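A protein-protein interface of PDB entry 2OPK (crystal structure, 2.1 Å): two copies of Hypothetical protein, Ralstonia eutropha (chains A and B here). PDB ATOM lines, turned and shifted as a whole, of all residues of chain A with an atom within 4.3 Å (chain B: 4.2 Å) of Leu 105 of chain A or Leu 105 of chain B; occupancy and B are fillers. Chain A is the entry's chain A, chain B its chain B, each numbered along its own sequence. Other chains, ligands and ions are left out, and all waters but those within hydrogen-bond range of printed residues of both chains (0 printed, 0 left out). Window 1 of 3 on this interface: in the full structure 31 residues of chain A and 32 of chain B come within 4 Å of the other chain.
Printed residues of chain B within 4 Å of Met 58 of chain A: Leu 105 (3.6 Å).
Leu 105 of chain A touches just these residues of chain B: Trp 56 (3.6 Å) and Leu 105 (3.3 Å).
Printed residues of chain A within 4 Å of Ile 33 of chain B: Trp 56 (3.6 Å).
Glu 34 of chain B touches none of the printed residues of chain A.
Of the printed residues of chain A, Trp 56 of chain B touches Leu 25, Ile 33 and Leu 105.
Of chain A, only Trp 56, Met 58 and Leu 105 come within 4 Å of Leu 105 of chain B.
The nearest printed residue of chain B that does not touch Met 58 of chain A is Met 58 of chain B (4.3 Å).
CD1 of Leu 25 of chain A touches CZ2 of Trp 56 of chain B, 3.7 Å away.
Ile 33 of chain A touches Trp 56 of chain B (CD1 to CB, 3.4 Å).
CD1 of Leu 25 of chain B touches CZ2 of Trp 56 of chain A, at 3.6 Å.
Ile 33 of chain B touches Trp 56 of chain A (CD1 to CB, 3.6 Å).
CH2 of Trp 56 of chain A touches CD1 of Leu 105 of chain B (3.6 Å).
Met 58 of chain A touches Leu 105 of chain B.
Trp 56 of chain B touches Leu 105 of chain A.
Leu 105 of chain A touches Leu 105 of chain B.
The backbone carbonyl oxygen (O) of Ile 33 of chain A is in hydrogen-bond range of the backbone NH (N) of Leu 25 of chain A (2.8 Å).
The backbone carbonyl oxygen (O) of Leu 105 of chain A lies within hydrogen-bond range of the backbone NH (N) of Met 58 of chain A, 3.0 Å away.
N of Leu 25 of chain B lies within hydrogen-bond range of O of Ile 33 of chain B (2.7 Å).
The backbone NH (N) of Met 58 of chain B is in hydrogen-bond range of the backbone carbonyl oxygen (O) of Leu 105 of chain B, at 2.9 Å.
Leu 25 of chain A touches Trp 56 of chain B, and with the chains exchanged Trp 56 of chain A touches Leu 25 of chain B.
Ile 33 of chain A touches Trp 56 of chain B, and with the chains exchanged Trp 56 of chain A touches Ile 33 of chain B.
Trp 56 of chain A touches Leu 105 of chain B, and with the chains exchanged Leu 105 of chain A touches Trp 56 of chain B.
Leu 105 of chain B touches its own counterpart, Leu 105 of chain A.
10 positions are printed for both chains.
Of the 8 pairs that touch across the chains among the printed residues, 7 have their exchanged pair printed and touching as well.
Of the 10 printed residues of chain A, 5 touch a printed residue of chain B.
Hydrophobic or aromatic side chains of chain A within 4 Å of the printed part of chain B: Leu 25, Ile 33, Trp 56, Met 58 and Leu 105.
Hydrophobic or aromatic side chains of chain B that line the printed part of chain A: Leu 25, Ile 33, Trp 56 and Leu 105.
Among the printed residues, no Asp or Glu carboxylate lies within 4 Å of a Lys or Arg side-chain nitrogen of the other chain.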
ATOM      1  N   LEU A  25     -19.255 -33.794  -0.083  1.00  0.00           N
ATOM      2  CA  LEU A  25     -19.602 -32.856  -1.150  1.00  0.00           C
ATOM      3  C   LEU A  25     -18.321 -32.302  -1.812  1.00  0.00           C
ATOM      4  O   LEU A  25     -18.297 -32.070  -3.017  1.00  0.00           O
ATOM      5  CB  LEU A  25     -20.437 -31.719  -0.573  1.00  0.00           C
ATOM      6  CG  LEU A  25     -21.696 -32.135   0.212  1.00  0.00           C
ATOM      7  CD1 LEU A  25     -22.456 -30.914   0.596  1.00  0.00           C
ATOM      8  CD2 LEU A  25     -22.602 -33.112  -0.573  1.00  0.00           C
ATOM      9  N   ILE A  33     -15.848 -31.149   2.966  1.00  0.00           N
ATOM     10  CA  ILE A  33     -17.193 -30.685   3.214  1.00  0.00           C
ATOM     11  C   ILE A  33     -18.064 -31.919   3.053  1.00  0.00           C
ATOM     12  O   ILE A  33     -17.960 -32.618   2.051  1.00  0.00           O
ATOM     13  CB  ILE A  33     -17.645 -29.596   2.212  1.00  0.00           C
ATOM     14  CG1 ILE A  33     -16.634 -28.422   2.171  1.00  0.00           C
ATOM     15  CG2 ILE A  33     -19.061 -29.085   2.586  1.00  0.00           C
ATOM     16  CD1 ILE A  33     -17.065 -27.248   1.231  1.00  0.00           C
ATOM     17  N   GLU A  34     -18.989 -32.148   3.980  1.00  0.00           N
ATOM     18  CA  GLU A  34     -19.869 -33.277   3.851  1.00  0.00           C
ATOM     19  C   GLU A  34     -21.298 -33.045   4.322  1.00  0.00           C
ATOM     20  O   GLU A  34     -21.542 -32.229   5.236  1.00  0.00           O
ATOM     21  CB  GLU A  34     -19.278 -34.476   4.632  1.00  0.00           C
ATOM     22  CG  GLU A  34     -19.174 -34.230   6.104  1.00  0.00           C
ATOM     23  CD  GLU A  34     -18.558 -35.410   6.884  1.00  0.00           C
ATOM     24  OE1 GLU A  34     -18.296 -36.457   6.252  1.00  0.00           O
ATOM     25  OE2 GLU A  34     -18.370 -35.249   8.128  1.00  0.00           O
ATOM     26  N   TRP A  56     -16.351 -27.470  11.613  1.00  0.00           N
ATOM     27  CA  TRP A  56     -17.351 -26.448  11.645  1.00  0.00           C
ATOM     28  C   TRP A  56     -18.595 -27.184  11.174  1.00  0.00           C
ATOM     29  O   TRP A  56     -18.615 -27.792  10.109  1.00  0.00           O
ATOM     30  CB  TRP A  56     -16.970 -25.248  10.750  1.00  0.00           C
ATOM     31  CG  TRP A  56     -17.996 -24.124  10.772  1.00  0.00           C
ATOM     32  CD1 TRP A  56     -17.938 -22.970  11.501  1.00  0.00           C
ATOM     33  CD2 TRP A  56     -19.218 -24.039  10.000  1.00  0.00           C
ATOM     34  NE1 TRP A  56     -19.047 -22.195  11.245  1.00  0.00           N
ATOM     35  CE2 TRP A  56     -19.838 -22.821  10.327  1.00  0.00           C
ATOM     36  CE3 TRP A  56     -19.829 -24.866   9.059  1.00  0.00           C
ATOM     37  CZ2 TRP A  56     -21.060 -22.438   9.786  1.00  0.00           C
ATOM     38  CZ3 TRP A  56     -21.036 -24.476   8.508  1.00  0.00           C
ATOM     39  CH2 TRP A  56     -21.643 -23.273   8.878  1.00  0.00           C
ATOM     40  N   VAL A  57     -19.635 -27.174  11.975  1.00  0.00           N
ATOM     41  CA  VAL A  57     -20.835 -27.943  11.625  1.00  0.00           C
ATOM     42  C   VAL A  57     -22.087 -27.143  11.949  1.00  0.00           C
ATOM     43  O   VAL A  57     -22.123 -26.442  12.959  1.00  0.00           O
ATOM     44  CB  VAL A  57     -20.846 -29.308  12.362  1.00  0.00           C
ATOM     45  CG1 VAL A  57     -20.865 -29.170  13.909  1.00  0.00           C
ATOM     46  CG2 VAL A  57     -21.967 -30.154  11.880  1.00  0.00           C
ATOM     47  N   MET A  58     -23.101 -27.272  11.078  1.00  0.00           N
ATOM     48  CA  MET A  58     -24.361 -26.584  11.188  1.00  0.00           C
ATOM     49  C   MET A  58     -25.547 -27.537  10.979  1.00  0.00           C
ATOM     50  O   MET A  58     -25.486 -28.442  10.157  1.00  0.00           O
ATOM     51  CB  MET A  58     -24.412 -25.518  10.099  1.00  0.00           C
ATOM     52  CG  MET A  58     -25.605 -24.562  10.194  1.00  0.00           C
ATOM     53  SD  MET A  58     -25.636 -23.145   8.738  1.00  0.00           S
ATOM     54  CE  MET A  58     -25.285 -24.434   7.304  1.00  0.00           C
ATOM     55  N   VAL A  60     -28.946 -27.834   9.272  1.00  0.00           N
ATOM     56  CA  VAL A  60     -29.695 -27.217   8.172  1.00  0.00           C
ATOM     57  C   VAL A  60     -31.194 -27.508   8.330  1.00  0.00           C
ATOM     58  O   VAL A  60     -32.031 -26.678   8.010  1.00  0.00           O
ATOM     59  CB  VAL A  60     -29.202 -27.780   6.829  1.00  0.00           C
ATOM     60  CG1 VAL A  60     -29.901 -27.065   5.700  1.00  0.00           C
ATOM     61  CG2 VAL A  60     -27.703 -27.573   6.734  1.00  0.00           C
ATOM     62  N   TRP A 104     -27.272 -32.183   8.355  1.00  0.00           N
ATOM     63  CA  TRP A 104     -26.151 -31.366   8.758  1.00  0.00           C
ATOM     64  C   TRP A 104     -25.221 -31.077   7.608  1.00  0.00           C
ATOM     65  O   TRP A 104     -25.087 -31.875   6.685  1.00  0.00           O
ATOM     66  CB  TRP A 104     -25.260 -32.106   9.753  1.00  0.00           C
ATOM     67  CG  TRP A 104     -25.879 -32.811  10.923  1.00  0.00           C
ATOM     68  CD1 TRP A 104     -26.589 -33.974  10.906  1.00  0.00           C
ATOM     69  CD2 TRP A 104     -25.728 -32.455  12.300  1.00  0.00           C
ATOM     70  NE1 TRP A 104     -26.904 -34.349  12.190  1.00  0.00           N
ATOM     71  CE2 TRP A 104     -26.384 -33.441  13.064  1.00  0.00           C
ATOM     72  CE3 TRP A 104     -25.127 -31.381  12.962  1.00  0.00           C
ATOM     73  CZ2 TRP A 104     -26.452 -33.383  14.466  1.00  0.00           C
ATOM     74  CZ3 TRP A 104     -25.186 -31.329  14.329  1.00  0.00           C
ATOM     75  CH2 TRP A 104     -25.850 -32.316  15.071  1.00  0.00           C
ATOM     76  N   LEU A 105     -24.511 -29.958   7.715  1.00  0.00           N
ATOM     77  CA  LEU A 105     -23.412 -29.646   6.809  1.00  0.00           C
ATOM     78  C   LEU A 105     -22.177 -29.491   7.677  1.00  0.00           C
ATOM     79  O   LEU A 105     -22.163 -28.667   8.561  1.00  0.00           O
ATOM     80  CB  LEU A 105     -23.659 -28.332   6.065  1.00  0.00           C
ATOM     81  CG  LEU A 105     -22.490 -27.992   5.145  1.00  0.00           C
ATOM     82  CD1 LEU A 105     -22.597 -28.818   3.866  1.00  0.00           C
ATOM     83  CD2 LEU A 105     -22.507 -26.585   4.849  1.00  0.00           C
ATOM     84  N   ALA A 106     -21.151 -30.280   7.418  1.00  0.00           N
ATOM     85  CA  ALA A 106     -19.924 -30.256   8.193  1.00  0.00           C
ATOM     86  C   ALA A 106     -18.724 -29.957   7.334  1.00  0.00           C
ATOM     87  O   ALA A 106     -18.610 -30.461   6.221  1.00  0.00           O
ATOM     88  CB  ALA A 106     -19.708 -31.614   8.866  1.00  0.00           C
ATOM     89  N   LEU B  25     -16.762 -16.765   9.183  1.00  0.00           N
ATOM     90  CA  LEU B  25     -17.101 -17.596  10.325  1.00  0.00           C
ATOM     91  C   LEU B  25     -15.895 -18.405  10.791  1.00  0.00           C
ATOM     92  O   LEU B  25     -15.735 -18.636  11.950  1.00  0.00           O
ATOM     93  CB  LEU B  25     -18.231 -18.551   9.924  1.00  0.00           C
ATOM     94  CG  LEU B  25     -19.505 -17.931   9.338  1.00  0.00           C
ATOM     95  CD1 LEU B  25     -20.538 -18.975   9.032  1.00  0.00           C
ATOM     96  CD2 LEU B  25     -20.069 -16.920  10.292  1.00  0.00           C
ATOM     97  N   ILE B  33     -14.533 -19.943   5.668  1.00  0.00           N
ATOM     98  CA  ILE B  33     -15.964 -20.185   5.717  1.00  0.00           C
ATOM     99  C   ILE B  33     -16.585 -18.848   6.043  1.00  0.00           C
ATOM    100  O   ILE B  33     -16.161 -18.176   6.994  1.00  0.00           O
ATOM    101  CB  ILE B  33     -16.351 -21.196   6.812  1.00  0.00           C
ATOM    102  CG1 ILE B  33     -15.603 -22.522   6.609  1.00  0.00           C
ATOM    103  CG2 ILE B  33     -17.855 -21.490   6.793  1.00  0.00           C
ATOM    104  CD1 ILE B  33     -15.885 -23.556   7.767  1.00  0.00           C
ATOM    105  N   GLU B  34     -17.593 -18.467   5.270  1.00  0.00           N
ATOM    106  CA  GLU B  34     -18.230 -17.179   5.451  1.00  0.00           C
ATOM    107  C   GLU B  34     -19.712 -17.218   5.135  1.00  0.00           C
ATOM    108  O   GLU B  34     -20.190 -18.031   4.349  1.00  0.00           O
ATOM    109  CB  GLU B  34     -17.565 -16.114   4.563  1.00  0.00           C
ATOM    110  CG  GLU B  34     -17.810 -16.315   3.077  1.00  0.00           C
ATOM    111  CD  GLU B  34     -17.077 -15.329   2.193  1.00  0.00           C
ATOM    112  OE1 GLU B  34     -16.585 -14.287   2.711  1.00  0.00           O
ATOM    113  OE2 GLU B  34     -17.014 -15.625   0.961  1.00  0.00           O
ATOM    114  N   TRP B  56     -17.285 -23.476  -2.675  1.00  0.00           N
ATOM    115  CA  TRP B  56     -18.463 -24.311  -2.469  1.00  0.00           C
ATOM    116  C   TRP B  56     -19.450 -23.334  -1.844  1.00  0.00           C
ATOM    117  O   TRP B  56     -19.134 -22.698  -0.848  1.00  0.00           O
ATOM    118  CB  TRP B  56     -18.149 -25.500  -1.537  1.00  0.00           C
ATOM    119  CG  TRP B  56     -19.371 -26.366  -1.308  1.00  0.00           C
ATOM    120  CD1 TRP B  56     -19.755 -27.444  -2.042  1.00  0.00           C
ATOM    121  CD2 TRP B  56     -20.393 -26.177  -0.320  1.00  0.00           C
ATOM    122  NE1 TRP B  56     -20.957 -27.941  -1.568  1.00  0.00           N
ATOM    123  CE2 TRP B  56     -21.370 -27.173  -0.525  1.00  0.00           C
ATOM    124  CE3 TRP B  56     -20.574 -25.269   0.727  1.00  0.00           C
ATOM    125  CZ2 TRP B  56     -22.494 -27.273   0.254  1.00  0.00           C
ATOM    126  CZ3 TRP B  56     -21.702 -25.386   1.509  1.00  0.00           C
ATOM    127  CH2 TRP B  56     -22.637 -26.370   1.273  1.00  0.00           C
ATOM    128  N   VAL B  57     -20.624 -23.176  -2.424  1.00  0.00           N
ATOM    129  CA  VAL B  57     -21.549 -22.131  -1.965  1.00  0.00           C
ATOM    130  C   VAL B  57     -22.966 -22.641  -1.991  1.00  0.00           C
ATOM    131  O   VAL B  57     -23.369 -23.315  -2.938  1.00  0.00           O
ATOM    132  CB  VAL B  57     -21.397 -20.823  -2.811  1.00  0.00           C
ATOM    133  CG1 VAL B  57     -21.660 -21.065  -4.331  1.00  0.00           C
ATOM    134  CG2 VAL B  57     -22.277 -19.724  -2.281  1.00  0.00           C
ATOM    135  N   MET B  58     -23.718 -22.320  -0.940  1.00  0.00           N
ATOM    136  CA  MET B  58     -25.081 -22.768  -0.798  1.00  0.00           C
ATOM    137  C   MET B  58     -26.019 -21.657  -0.356  1.00  0.00           C
ATOM    138  O   MET B  58     -25.673 -20.847   0.496  1.00  0.00           O
ATOM    139  CB  MET B  58     -25.141 -23.880   0.260  1.00  0.00           C
ATOM    140  CG  MET B  58     -26.506 -24.588   0.377  1.00  0.00           C
ATOM    141  SD  MET B  58     -26.484 -26.033   1.731  1.00  0.00           S
ATOM    142  CE  MET B  58     -25.824 -25.077   3.091  1.00  0.00           C
ATOM    143  N   VAL B  60     -28.994 -20.690   1.863  1.00  0.00           N
ATOM    144  CA  VAL B  60     -29.558 -21.191   3.117  1.00  0.00           C
ATOM    145  C   VAL B  60     -30.938 -20.580   3.391  1.00  0.00           C
ATOM    146  O   VAL B  60     -31.802 -21.223   4.012  1.00  0.00           O
ATOM    147  CB  VAL B  60     -28.572 -20.931   4.285  1.00  0.00           C
ATOM    148  CG1 VAL B  60     -28.972 -21.689   5.479  1.00  0.00           C
ATOM    149  CG2 VAL B  60     -27.189 -21.407   3.915  1.00  0.00           C
ATOM    150  N   TRP B 104     -26.297 -16.868   2.358  1.00  0.00           N
ATOM    151  CA  TRP B 104     -25.497 -17.946   1.768  1.00  0.00           C
ATOM    152  C   TRP B 104     -24.428 -18.391   2.737  1.00  0.00           C
ATOM    153  O   TRP B 104     -24.030 -17.633   3.620  1.00  0.00           O
ATOM    154  CB  TRP B 104     -24.716 -17.476   0.570  1.00  0.00           C
ATOM    155  CG  TRP B 104     -25.413 -16.645  -0.474  1.00  0.00           C
ATOM    156  CD1 TRP B 104     -25.868 -15.388  -0.335  1.00  0.00           C
ATOM    157  CD2 TRP B 104     -25.668 -17.022  -1.835  1.00  0.00           C
ATOM    158  NE1 TRP B 104     -26.401 -14.942  -1.520  1.00  0.00           N
ATOM    159  CE2 TRP B 104     -26.299 -15.931  -2.457  1.00  0.00           C
ATOM    160  CE3 TRP B 104     -25.441 -18.184  -2.580  1.00  0.00           C
ATOM    161  CZ2 TRP B 104     -26.677 -15.955  -3.805  1.00  0.00           C
ATOM    162  CZ3 TRP B 104     -25.799 -18.215  -3.913  1.00  0.00           C
ATOM    163  CH2 TRP B 104     -26.426 -17.116  -4.515  1.00  0.00           C
ATOM    164  N   LEU B 105     -23.950 -19.610   2.521  1.00  0.00           N
ATOM    165  CA  LEU B 105     -22.781 -20.144   3.221  1.00  0.00           C
ATOM    166  C   LEU B 105     -21.794 -20.466   2.136  1.00  0.00           C
ATOM    167  O   LEU B 105     -22.141 -21.158   1.167  1.00  0.00           O
ATOM    168  CB  LEU B 105     -23.136 -21.413   3.992  1.00  0.00           C
ATOM    169  CG  LEU B 105     -21.995 -22.001   4.824  1.00  0.00           C
ATOM    170  CD1 LEU B 105     -21.611 -21.085   5.996  1.00  0.00           C
ATOM    171  CD2 LEU B 105     -22.429 -23.345   5.336  1.00  0.00           C
ATOM    172  N   ALA B 106     -20.583 -19.933   2.256  1.00  0.00           N
ATOM    173  CA  ALA B 106     -19.573 -20.086   1.236  1.00  0.00           C
ATOM    174  C   ALA B 106     -18.256 -20.571   1.831  1.00  0.00           C
ATOM    175  O   ALA B 106     -17.842 -20.119   2.912  1.00  0.00           O
ATOM    176  CB  ALA B 106     -19.385 -18.776   0.478  1.00  0.00           C
